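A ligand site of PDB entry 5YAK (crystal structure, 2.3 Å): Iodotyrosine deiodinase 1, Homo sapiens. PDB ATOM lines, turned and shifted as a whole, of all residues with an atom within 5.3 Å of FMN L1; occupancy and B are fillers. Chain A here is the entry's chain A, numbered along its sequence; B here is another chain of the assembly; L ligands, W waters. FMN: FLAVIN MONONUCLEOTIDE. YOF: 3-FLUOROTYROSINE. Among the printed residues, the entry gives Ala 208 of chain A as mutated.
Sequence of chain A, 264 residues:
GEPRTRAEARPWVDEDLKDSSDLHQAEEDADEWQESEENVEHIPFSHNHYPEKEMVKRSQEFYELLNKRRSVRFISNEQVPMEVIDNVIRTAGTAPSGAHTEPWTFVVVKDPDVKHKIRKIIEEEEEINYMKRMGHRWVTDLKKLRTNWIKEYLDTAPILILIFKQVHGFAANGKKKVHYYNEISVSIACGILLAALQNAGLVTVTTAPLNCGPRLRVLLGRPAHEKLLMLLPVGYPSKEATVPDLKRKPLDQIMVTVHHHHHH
The backbone NH of Ser 71 lies within hydrogen-bond range of an oxygen (O3P) of FMN L1. An oxygen (O2P) of FMN L1 is in hydrogen-bond range of the side-chain hydroxyl of Ser 71 (2.5 Å). O2 of FMN L1 is in hydrogen-bond range of NE of Arg 73 (2.8 Å). An oxygen (O3P) of FMN L1 lies within salt-bridge range of the guanidinium group (NE) of Arg 70 (2.9 Å). NH2 of Arg 248 is in salt-bridge range of O1P of FMN L1. The backbone NH of Ala 208 lies within hydrogen-bond range of an oxygen (O4) of FMN L1 (3.0 Å). The backbone NH of Ser 97 of chain B is in hydrogen-bond range of an oxygen (O3') of FMN L1, 3.1 Å away. O2P of FMN L1 lies within salt-bridge range of NH2 of Arg 69. The backbone NH of Ala 99 of chain B is in hydrogen-bond range of an oxygen (OH) of YOF L2 (3.2 Å). The side-chain amino group (NZ) of Lys 151 lies within salt-bridge range of an oxygen (OXT) of YOF L2 (2.6 Å). The side-chain carboxylate (OE2) of Glu 126 is in salt-bridge range of a nitrogen (N) of YOF L2 (3.0 Å).
O4 of FMN L1 sits at hydrogen-bond distance from N of YOF L2 (2.8 Å).
O of Arg 69 lies within hydrogen-bond range of NH2 of Arg 248, 3.0 Å away. The guanidinium group (NH2) of Arg 248 is in hydrogen-bond range of the backbone carbonyl oxygen (O) of Thr 94 of chain B. The guanidinium group (NH2) of Arg 69 lies within hydrogen-bond range of the backbone carbonyl oxygen (O) of Thr 94 of chain B, 2.9 Å away. OG of Ser 185 of chain B is in hydrogen-bond range of O of Tyr 181 of chain B (2.7 Å). OG of Ser 185 of chain B is in hydrogen-bond range of N of Gly 98 of chain B, 3.1 Å away.
O of Thr 206 lies close to N10 of FMN L1, at 2.8 Å. Residues that only touch FMN L1: Leu 145, Thr 147, Val 205, Thr 207, Leu 246, Pro 96 of chain B, Gly 98 of chain B, His 100 of chain B, Tyr 181 of chain B, Ile 184 of chain B and Ser 185 of chain B. Of the 27 residues printed, 19 come within 4 Å of FMN L1.
Water W4 lies within hydrogen-bond range of O3P of FMN L1 (2.4 Å), O of Ser 71 (2.8 Å) and NH2 of Arg 70 (3.1 Å). Water W2 lies within hydrogen-bond range of an oxygen (O2) of FMN L1 (2.7 Å), the side-chain hydroxyl of Tyr 153 (2.8 Å) and the side-chain amino group of Lys 151 (3.1 Å). Water W1 lies within hydrogen-bond range of an oxygen (O1P) of FMN L1 (2.7 Å), the backbone carbonyl oxygen (O) of Ala 95 of chain B (2.8 Å) and the guanidinium group (NE) of Arg 248 (3.0 Å). Water W5 bridges the guanidinium group of Arg 73 (2.7 Å) and an oxygen (O4') of FMN L1 (2.9 Å).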
ATOM      1  N   ARG A  69       1.337  37.867  24.898  1.00  0.00           N
ATOM      2  CA  ARG A  69       0.961  36.519  25.363  1.00  0.00           C
ATOM      3  C   ARG A  69       1.143  35.449  24.313  1.00  0.00           C
ATOM      4  O   ARG A  69       0.622  35.530  23.207  1.00  0.00           O
ATOM      5  CB  ARG A  69      -0.507  36.451  25.789  1.00  0.00           C
ATOM      6  CG  ARG A  69      -0.821  35.236  26.675  1.00  0.00           C
ATOM      7  CD  ARG A  69      -2.292  34.789  26.543  1.00  0.00           C
ATOM      8  NE  ARG A  69      -2.636  34.526  25.146  1.00  0.00           N
ATOM      9  CZ  ARG A  69      -2.250  33.465  24.454  1.00  0.00           C
ATOM     10  NH1 ARG A  69      -1.559  32.488  25.053  1.00  0.00           N
ATOM     11  NH2 ARG A  69      -2.607  33.349  23.185  1.00  0.00           N
ATOM     12  N   ARG A  70       1.925  34.441  24.668  1.00  0.00           N
ATOM     13  CA  ARG A  70       2.080  33.243  23.872  1.00  0.00           C
ATOM     14  C   ARG A  70       1.967  32.029  24.776  1.00  0.00           C
ATOM     15  O   ARG A  70       2.362  32.073  25.961  1.00  0.00           O
ATOM     16  CB  ARG A  70       3.442  33.208  23.175  1.00  0.00           C
ATOM     17  CG  ARG A  70       3.651  34.345  22.179  1.00  0.00           C
ATOM     18  CD  ARG A  70       2.696  34.305  20.990  1.00  0.00           C
ATOM     19  NE  ARG A  70       2.605  32.981  20.407  1.00  0.00           N
ATOM     20  CZ  ARG A  70       3.452  32.436  19.540  1.00  0.00           C
ATOM     21  NH1 ARG A  70       4.505  33.096  19.125  1.00  0.00           N
ATOM     22  NH2 ARG A  70       3.248  31.214  19.101  1.00  0.00           N
ATOM     23  N   SER A  71       1.454  30.925  24.236  1.00  0.00           N
ATOM     24  CA  SER A  71       1.385  29.681  25.025  1.00  0.00           C
ATOM     25  C   SER A  71       2.822  29.220  25.163  1.00  0.00           C
ATOM     26  O   SER A  71       3.504  29.031  24.154  1.00  0.00           O
ATOM     27  CB  SER A  71       0.488  28.617  24.348  1.00  0.00           C
ATOM     28  OG  SER A  71      -0.892  29.018  24.349  1.00  0.00           O
ATOM     29  N   ARG A  73       5.375  26.375  26.672  1.00  0.00           N
ATOM     30  CA  ARG A  73       5.404  25.004  27.122  1.00  0.00           C
ATOM     31  C   ARG A  73       6.700  24.639  27.867  1.00  0.00           C
ATOM     32  O   ARG A  73       6.948  23.463  28.120  1.00  0.00           O
ATOM     33  CB  ARG A  73       5.200  24.071  25.932  1.00  0.00           C
ATOM     34  CG  ARG A  73       3.845  24.253  25.311  1.00  0.00           C
ATOM     35  CD  ARG A  73       3.664  23.438  24.069  1.00  0.00           C
ATOM     36  NE  ARG A  73       2.297  23.595  23.651  1.00  0.00           N
ATOM     37  CZ  ARG A  73       1.894  24.410  22.688  1.00  0.00           C
ATOM     38  NH1 ARG A  73       2.760  25.148  21.957  1.00  0.00           N
ATOM     39  NH2 ARG A  73       0.596  24.498  22.445  1.00  0.00           N
ATOM     40  N   GLU A 126      -2.012  10.744  27.635  1.00  0.00           N
ATOM     41  CA  GLU A 126      -1.682  11.406  26.359  1.00  0.00           C
ATOM     42  C   GLU A 126      -0.919  10.487  25.410  1.00  0.00           C
ATOM     43  O   GLU A 126      -1.123  10.535  24.183  1.00  0.00           O
ATOM     44  CB  GLU A 126      -0.904  12.713  26.585  1.00  0.00           C
ATOM     45  CG  GLU A 126      -1.739  13.797  27.269  1.00  0.00           C
ATOM     46  CD  GLU A 126      -2.714  14.525  26.352  1.00  0.00           C
ATOM     47  OE1 GLU A 126      -3.088  13.995  25.295  1.00  0.00           O
ATOM     48  OE2 GLU A 126      -3.094  15.657  26.688  1.00  0.00           O
ATOM     49  N   LEU A 145       3.161  22.321  16.143  1.00  0.00           N
ATOM     50  CA  LEU A 145       3.334  22.782  17.508  1.00  0.00           C
ATOM     51  C   LEU A 145       4.387  21.930  18.179  1.00  0.00           C
ATOM     52  O   LEU A 145       4.892  22.320  19.221  1.00  0.00           O
ATOM     53  CB  LEU A 145       2.027  22.679  18.295  1.00  0.00           C
ATOM     54  CG  LEU A 145       0.809  23.425  17.742  1.00  0.00           C
ATOM     55  CD1 LEU A 145      -0.443  23.222  18.583  1.00  0.00           C
ATOM     56  CD2 LEU A 145       1.110  24.909  17.637  1.00  0.00           C
ATOM     57  N   THR A 147       4.133  19.275  19.934  1.00  0.00           N
ATOM     58  CA  THR A 147       3.679  18.611  21.156  1.00  0.00           C
ATOM     59  C   THR A 147       3.712  17.067  21.035  1.00  0.00           C
ATOM     60  O   THR A 147       3.514  16.508  19.963  1.00  0.00           O
ATOM     61  CB  THR A 147       2.229  19.014  21.441  1.00  0.00           C
ATOM     62  OG1 THR A 147       1.456  18.822  20.242  1.00  0.00           O
ATOM     63  CG2 THR A 147       2.153  20.481  21.838  1.00  0.00           C
ATOM     64  N   LYS A 151       5.350  15.806  29.174  1.00  0.00           N
ATOM     65  CA  LYS A 151       4.847  17.070  29.711  1.00  0.00           C
ATOM     66  C   LYS A 151       5.668  17.440  30.913  1.00  0.00           C
ATOM     67  O   LYS A 151       5.188  17.476  32.039  1.00  0.00           O
ATOM     68  CB  LYS A 151       3.360  16.976  30.057  1.00  0.00           C
ATOM     69  CG  LYS A 151       2.458  16.532  28.894  1.00  0.00           C
ATOM     70  CD  LYS A 151       2.539  17.457  27.689  1.00  0.00           C
ATOM     71  CE  LYS A 151       1.474  17.118  26.670  1.00  0.00           C
ATOM     72  NZ  LYS A 151       1.701  17.741  25.335  1.00  0.00           N
ATOM     73  N   TYR A 153       6.709  20.234  31.908  1.00  0.00           N
ATOM     74  CA  TYR A 153       6.254  21.412  32.637  1.00  0.00           C
ATOM     75  C   TYR A 153       5.431  21.076  33.878  1.00  0.00           C
ATOM     76  O   TYR A 153       5.344  21.892  34.808  1.00  0.00           O
ATOM     77  CB  TYR A 153       5.519  22.375  31.699  1.00  0.00           C
ATOM     78  CG  TYR A 153       4.344  21.795  30.941  1.00  0.00           C
ATOM     79  CD1 TYR A 153       4.420  21.603  29.565  1.00  0.00           C
ATOM     80  CD2 TYR A 153       3.150  21.507  31.576  1.00  0.00           C
ATOM     81  CE1 TYR A 153       3.341  21.103  28.853  1.00  0.00           C
ATOM     82  CE2 TYR A 153       2.072  20.999  30.871  1.00  0.00           C
ATOM     83  CZ  TYR A 153       2.164  20.803  29.518  1.00  0.00           C
ATOM     84  OH  TYR A 153       1.061  20.320  28.818  1.00  0.00           O
ATOM     85  N   VAL A 205       0.445  27.750  29.624  1.00  0.00           N
ATOM     86  CA  VAL A 205      -0.187  27.225  28.405  1.00  0.00           C
ATOM     87  C   VAL A 205      -1.490  26.549  28.763  1.00  0.00           C
ATOM     88  O   VAL A 205      -1.583  25.784  29.731  1.00  0.00           O
ATOM     89  CB  VAL A 205       0.715  26.250  27.681  1.00  0.00           C
ATOM     90  CG1 VAL A 205       1.351  25.289  28.661  1.00  0.00           C
ATOM     91  CG2 VAL A 205      -0.038  25.526  26.565  1.00  0.00           C
ATOM     92  N   THR A 206      -2.507  26.869  27.990  1.00  0.00           N
ATOM     93  CA  THR A 206      -3.838  26.379  28.215  1.00  0.00           C
ATOM     94  C   THR A 206      -3.858  24.951  27.726  1.00  0.00           C
ATOM     95  O   THR A 206      -3.711  24.710  26.518  1.00  0.00           O
ATOM     96  CB  THR A 206      -4.844  27.230  27.415  1.00  0.00           C
ATOM     97  OG1 THR A 206      -4.859  28.531  27.961  1.00  0.00           O
ATOM     98  CG2 THR A 206      -6.224  26.662  27.517  1.00  0.00           C
ATOM     99  N   THR A 207      -4.028  23.992  28.628  1.00  0.00           N
ATOM    100  CA  THR A 207      -4.116  22.590  28.176  1.00  0.00           C
ATOM    101  C   THR A 207      -5.414  21.882  28.506  1.00  0.00           C
ATOM    102  O   THR A 207      -6.043  22.142  29.529  1.00  0.00           O
ATOM    103  CB  THR A 207      -2.940  21.746  28.693  1.00  0.00           C
ATOM    104  OG1 THR A 207      -3.128  21.497  30.089  1.00  0.00           O
ATOM    105  CG2 THR A 207      -1.631  22.456  28.478  1.00  0.00           C
ATOM    106  N   ALA A 208      -5.771  20.939  27.638  1.00  0.00           N
ATOM    107  CA  ALA A 208      -6.947  20.108  27.796  1.00  0.00           C
ATOM    108  C   ALA A 208      -6.493  18.639  27.784  1.00  0.00           C
ATOM    109  O   ALA A 208      -6.467  17.990  26.739  1.00  0.00           O
ATOM    110  CB  ALA A 208      -7.941  20.358  26.678  1.00  0.00           C
ATOM    111  N   PRO A 209      -6.125  18.112  28.962  1.00  0.00           N
ATOM    112  CA  PRO A 209      -5.654  16.731  29.044  1.00  0.00           C
ATOM    113  C   PRO A 209      -6.802  15.715  28.857  1.00  0.00           C
ATOM    114  O   PRO A 209      -7.439  15.281  29.825  1.00  0.00           O
ATOM    115  CB  PRO A 209      -5.035  16.672  30.436  1.00  0.00           C
ATOM    116  CG  PRO A 209      -5.741  17.736  31.227  1.00  0.00           C
ATOM    117  CD  PRO A 209      -6.164  18.800  30.260  1.00  0.00           C
ATOM    118  N   LEU A 246       3.987  31.336  14.888  1.00  0.00           N
ATOM    119  CA  LEU A 246       2.631  31.371  14.376  1.00  0.00           C
ATOM    120  C   LEU A 246       2.206  32.816  14.250  1.00  0.00           C
ATOM    121  O   LEU A 246       2.605  33.664  15.052  1.00  0.00           O
ATOM    122  CB  LEU A 246       1.636  30.677  15.329  1.00  0.00           C
ATOM    123  CG  LEU A 246       1.993  29.285  15.853  1.00  0.00           C
ATOM    124  CD1 LEU A 246       1.044  28.906  16.971  1.00  0.00           C
ATOM    125  CD2 LEU A 246       1.990  28.244  14.754  1.00  0.00           C
ATOM    126  N   ARG A 248      -1.205  35.477  13.908  1.00  0.00           N
ATOM    127  CA  ARG A 248      -2.625  35.719  14.061  1.00  0.00           C
ATOM    128  C   ARG A 248      -3.256  36.340  12.804  1.00  0.00           C
ATOM    129  O   ARG A 248      -2.591  37.022  12.017  1.00  0.00           O
ATOM    130  CB  ARG A 248      -2.844  36.570  15.317  1.00  0.00           C
ATOM    131  CG  ARG A 248      -2.640  35.715  16.576  1.00  0.00           C
ATOM    132  CD  ARG A 248      -2.330  36.490  17.833  1.00  0.00           C
ATOM    133  NE  ARG A 248      -2.079  35.580  18.925  1.00  0.00           N
ATOM    134  CZ  ARG A 248      -1.368  35.856  20.001  1.00  0.00           C
ATOM    135  NH1 ARG A 248      -0.824  37.050  20.139  1.00  0.00           N
ATOM    136  NH2 ARG A 248      -1.191  34.927  20.922  1.00  0.00           N
ATOM    137  N   THR B  94      -6.292  37.754  20.170  1.00  0.00           N
ATOM    138  CA  THR B  94      -5.036  37.251  20.731  1.00  0.00           C
ATOM    139  C   THR B  94      -5.180  36.001  21.597  1.00  0.00           C
ATOM    140  O   THR B  94      -4.185  35.512  22.141  1.00  0.00           O
ATOM    141  CB  THR B  94      -4.347  38.314  21.639  1.00  0.00           C
ATOM    142  OG1 THR B  94      -5.133  38.558  22.827  1.00  0.00           O
ATOM    143  CG2 THR B  94      -4.139  39.627  20.855  1.00  0.00           C
ATOM    144  N   ALA B  95      -6.428  35.571  21.812  1.00  0.00           N
ATOM    145  CA  ALA B  95      -6.728  34.374  22.587  1.00  0.00           C
ATOM    146  C   ALA B  95      -5.994  33.156  22.102  1.00  0.00           C
ATOM    147  O   ALA B  95      -5.764  33.021  20.910  1.00  0.00           O
ATOM    148  CB  ALA B  95      -8.211  34.056  22.526  1.00  0.00           C
ATOM    149  N   PRO B  96      -5.722  32.214  23.015  1.00  0.00           N
ATOM    150  CA  PRO B  96      -5.311  30.885  22.599  1.00  0.00           C
ATOM    151  C   PRO B  96      -6.444  30.148  21.875  1.00  0.00           C
ATOM    152  O   PRO B  96      -7.606  30.521  22.034  1.00  0.00           O
ATOM    153  CB  PRO B  96      -4.963  30.205  23.900  1.00  0.00           C
ATOM    154  CG  PRO B  96      -5.802  30.861  24.907  1.00  0.00           C
ATOM    155  CD  PRO B  96      -5.905  32.291  24.467  1.00  0.00           C
ATOM    156  N   SER B  97      -6.127  29.139  21.085  1.00  0.00           N
ATOM    157  CA  SER B  97      -7.165  28.324  20.437  1.00  0.00           C
ATOM    158  C   SER B  97      -6.632  26.926  20.148  1.00  0.00           C
ATOM    159  O   SER B  97      -5.457  26.753  19.848  1.00  0.00           O
ATOM    160  CB  SER B  97      -7.714  28.967  19.154  1.00  0.00           C
ATOM    161  OG  SER B  97      -6.756  29.005  18.089  1.00  0.00           O
ATOM    162  N   GLY B  98      -7.511  25.944  20.253  1.00  0.00           N
ATOM    163  CA  GLY B  98      -7.172  24.549  19.951  1.00  0.00           C
ATOM    164  C   GLY B  98      -6.460  24.380  18.628  1.00  0.00           C
ATOM    165  O   GLY B  98      -6.998  24.705  17.595  1.00  0.00           O
ATOM    166  N   ALA B  99      -5.233  23.872  18.693  1.00  0.00           N
ATOM    167  CA  ALA B  99      -4.394  23.654  17.507  1.00  0.00           C
ATOM    168  C   ALA B  99      -4.223  24.917  16.652  1.00  0.00           C
ATOM    169  O   ALA B  99      -4.079  24.821  15.432  1.00  0.00           O
ATOM    170  CB  ALA B  99      -4.924  22.513  16.657  1.00  0.00           C
ATOM    171  N   HIS B 100      -4.250  26.098  17.278  1.00  0.00           N
ATOM    172  CA  HIS B 100      -4.090  27.363  16.543  1.00  0.00           C
ATOM    173  C   HIS B 100      -5.044  27.444  15.361  1.00  0.00           C
ATOM    174  O   HIS B 100      -4.622  27.625  14.217  1.00  0.00           O
ATOM    175  CB  HIS B 100      -2.640  27.561  16.026  1.00  0.00           C
ATOM    176  CG  HIS B 100      -2.394  28.947  15.493  1.00  0.00           C
ATOM    177  ND1 HIS B 100      -2.807  30.076  16.148  1.00  0.00           N
ATOM    178  CD2 HIS B 100      -1.810  29.363  14.348  1.00  0.00           C
ATOM    179  CE1 HIS B 100      -2.498  31.144  15.435  1.00  0.00           C
ATOM    180  NE2 HIS B 100      -1.896  30.731  14.338  1.00  0.00           N
ATOM    181  N   TYR B 181     -11.740  21.954  20.104  1.00  0.00           N
ATOM    182  CA  TYR B 181     -12.152  22.744  21.246  1.00  0.00           C
ATOM    183  C   TYR B 181     -12.661  24.113  20.796  1.00  0.00           C
ATOM    184  O   TYR B 181     -12.277  25.102  21.401  1.00  0.00           O
ATOM    185  CB  TYR B 181     -10.994  22.948  22.233  1.00  0.00           C
ATOM    186  CG  TYR B 181     -10.487  21.652  22.778  1.00  0.00           C
ATOM    187  CD1 TYR B 181      -9.242  21.169  22.391  1.00  0.00           C
ATOM    188  CD2 TYR B 181     -11.269  20.865  23.625  1.00  0.00           C
ATOM    189  CE1 TYR B 181      -8.776  19.966  22.836  1.00  0.00           C
ATOM    190  CE2 TYR B 181     -10.794  19.652  24.088  1.00  0.00           C
ATOM    191  CZ  TYR B 181      -9.554  19.201  23.676  1.00  0.00           C
ATOM    192  OH  TYR B 181      -9.035  17.977  24.097  1.00  0.00           O
ATOM    193  N   ILE B 184     -14.873  26.169  23.493  1.00  0.00           N
ATOM    194  CA  ILE B 184     -14.102  26.650  24.571  1.00  0.00           C
ATOM    195  C   ILE B 184     -13.159  27.798  24.169  1.00  0.00           C
ATOM    196  O   ILE B 184     -12.955  28.732  24.932  1.00  0.00           O
ATOM    197  CB  ILE B 184     -13.343  25.538  25.243  1.00  0.00           C
ATOM    198  CG1 ILE B 184     -14.345  24.585  25.945  1.00  0.00           C
ATOM    199  CG2 ILE B 184     -12.337  26.093  26.243  1.00  0.00           C
ATOM    200  CD1 ILE B 184     -13.705  23.278  26.361  1.00  0.00           C
ATOM    201  N   SER B 185     -12.531  27.645  23.021  1.00  0.00           N
ATOM    202  CA  SER B 185     -11.626  28.602  22.448  1.00  0.00           C
ATOM    203  C   SER B 185     -12.368  29.921  22.271  1.00  0.00           C
ATOM    204  O   SER B 185     -11.894  30.981  22.699  1.00  0.00           O
ATOM    205  CB  SER B 185     -11.072  28.090  21.102  1.00  0.00           C
ATOM    206  OG  SER B 185     -10.292  26.884  21.233  1.00  0.00           O
ATOM    207  N   ILE B 188     -13.176  31.543  25.598  1.00  0.00           N
ATOM    208  CA  ILE B 188     -12.007  32.135  26.241  1.00  0.00           C
ATOM    209  C   ILE B 188     -11.725  33.549  25.636  1.00  0.00           C
ATOM    210  O   ILE B 188     -11.404  34.506  26.349  1.00  0.00           O
ATOM    211  CB  ILE B 188     -10.805  31.263  26.071  1.00  0.00           C
ATOM    212  CG1 ILE B 188     -10.826  30.117  27.075  1.00  0.00           C
ATOM    213  CG2 ILE B 188      -9.521  32.069  26.234  1.00  0.00           C
ATOM    214  CD1 ILE B 188      -9.736  29.086  26.810  1.00  0.00           C
HETATM  215  N1  FMN L   1      -1.721  23.338  24.066  1.00  0.00           N
HETATM  216  C2  FMN L   1      -1.178  22.180  24.467  1.00  0.00           C
HETATM  217  O2  FMN L   1       0.055  22.087  24.388  1.00  0.00           O
HETATM  218  N3  FMN L   1      -1.919  21.107  24.850  1.00  0.00           N
HETATM  219  C4  FMN L   1      -3.274  21.163  24.927  1.00  0.00           C
HETATM  220  O4  FMN L   1      -4.009  20.224  25.316  1.00  0.00           O
HETATM  221  C4A FMN L   1      -3.919  22.412  24.519  1.00  0.00           C
HETATM  222  N5  FMN L   1      -5.255  22.521  24.594  1.00  0.00           N
HETATM  223  C5A FMN L   1      -5.841  23.700  24.297  1.00  0.00           C
HETATM  224  C6  FMN L   1      -7.214  23.779  24.409  1.00  0.00           C
HETATM  225  C7  FMN L   1      -7.845  24.968  24.136  1.00  0.00           C
HETATM  226  C7M FMN L   1      -9.320  25.111  24.305  1.00  0.00           C
HETATM  227  C8  FMN L   1      -7.050  26.150  23.765  1.00  0.00           C
HETATM  228  C8M FMN L   1      -7.768  27.433  23.502  1.00  0.00           C
HETATM  229  C9  FMN L   1      -5.691  26.058  23.591  1.00  0.00           C
HETATM  230  C9A FMN L   1      -5.019  24.876  23.862  1.00  0.00           C
HETATM  231  N10 FMN L   1      -3.607  24.774  23.728  1.00  0.00           N
HETATM  232  C10 FMN L   1      -3.037  23.536  24.085  1.00  0.00           C
HETATM  233  C1' FMN L   1      -2.762  25.905  23.329  1.00  0.00           C
HETATM  234  C2' FMN L   1      -2.886  26.151  21.808  1.00  0.00           C
HETATM  235  O2' FMN L   1      -2.142  25.102  21.142  1.00  0.00           O
HETATM  236  C3' FMN L   1      -2.353  27.575  21.451  1.00  0.00           C
HETATM  237  O3' FMN L   1      -3.234  28.599  21.954  1.00  0.00           O
HETATM  238  C4' FMN L   1      -2.155  27.831  19.963  1.00  0.00           C
HETATM  239  O4' FMN L   1      -1.161  26.972  19.382  1.00  0.00           O
HETATM  240  C5' FMN L   1      -1.807  29.286  19.610  1.00  0.00           C
HETATM  241  O5' FMN L   1      -0.631  29.710  20.282  1.00  0.00           O
HETATM  242  P   FMN L   1      -0.671  30.952  21.304  1.00  0.00           P
HETATM  243  O1P FMN L   1      -1.357  32.031  20.505  1.00  0.00           O
HETATM  244  O2P FMN L   1      -1.502  30.526  22.514  1.00  0.00           O
HETATM  245  O3P FMN L   1       0.803  31.085  21.691  1.00  0.00           O
HETATM  246  N   YOF L   2      -3.587  17.595  24.470  1.00  0.00           N
HETATM  247  CA  YOF L   2      -2.451  17.205  23.602  1.00  0.00           C
HETATM  248  C   YOF L   2      -1.204  17.669  24.241  1.00  0.00           C
HETATM  249  O   YOF L   2      -1.274  18.329  25.327  1.00  0.00           O
HETATM  250  OXT YOF L   2      -0.158  17.467  23.570  1.00  0.00           O
HETATM  251  CB  YOF L   2      -2.236  17.854  22.237  1.00  0.00           C
HETATM  252  CG  YOF L   2      -2.955  19.125  21.876  1.00  0.00           C
HETATM  253  CD1 YOF L   2      -2.557  20.457  21.567  1.00  0.00           C
HETATM  254  CD2 YOF L   2      -4.234  18.736  21.772  1.00  0.00           C
HETATM  255  CE1 YOF L   2      -3.599  21.387  21.193  1.00  0.00           C
HETATM  256  CE2 YOF L   2      -5.183  19.624  21.420  1.00  0.00           C
HETATM  257  CZ  YOF L   2      -4.896  20.903  21.168  1.00  0.00           C
HETATM  258  OH  YOF L   2      -6.013  21.551  20.795  1.00  0.00           O
HETATM  259  F   YOF L   2      -3.478  22.700  20.845  1.00  0.00           F
HETATM  260  O   HOH W   1      -3.542  32.927  19.195  1.00  0.00           O
HETATM  261  O   HOH W   2       1.543  20.716  26.132  1.00  0.00           O
HETATM  262  O   HOH W   3      -0.434  32.266  18.214  1.00  0.00           O
HETATM  263  O   HOH W   4       2.623  29.486  21.552  1.00  0.00           O
HETATM  264  O   HOH W   5       1.525  27.007  20.384  1.00  0.00           O
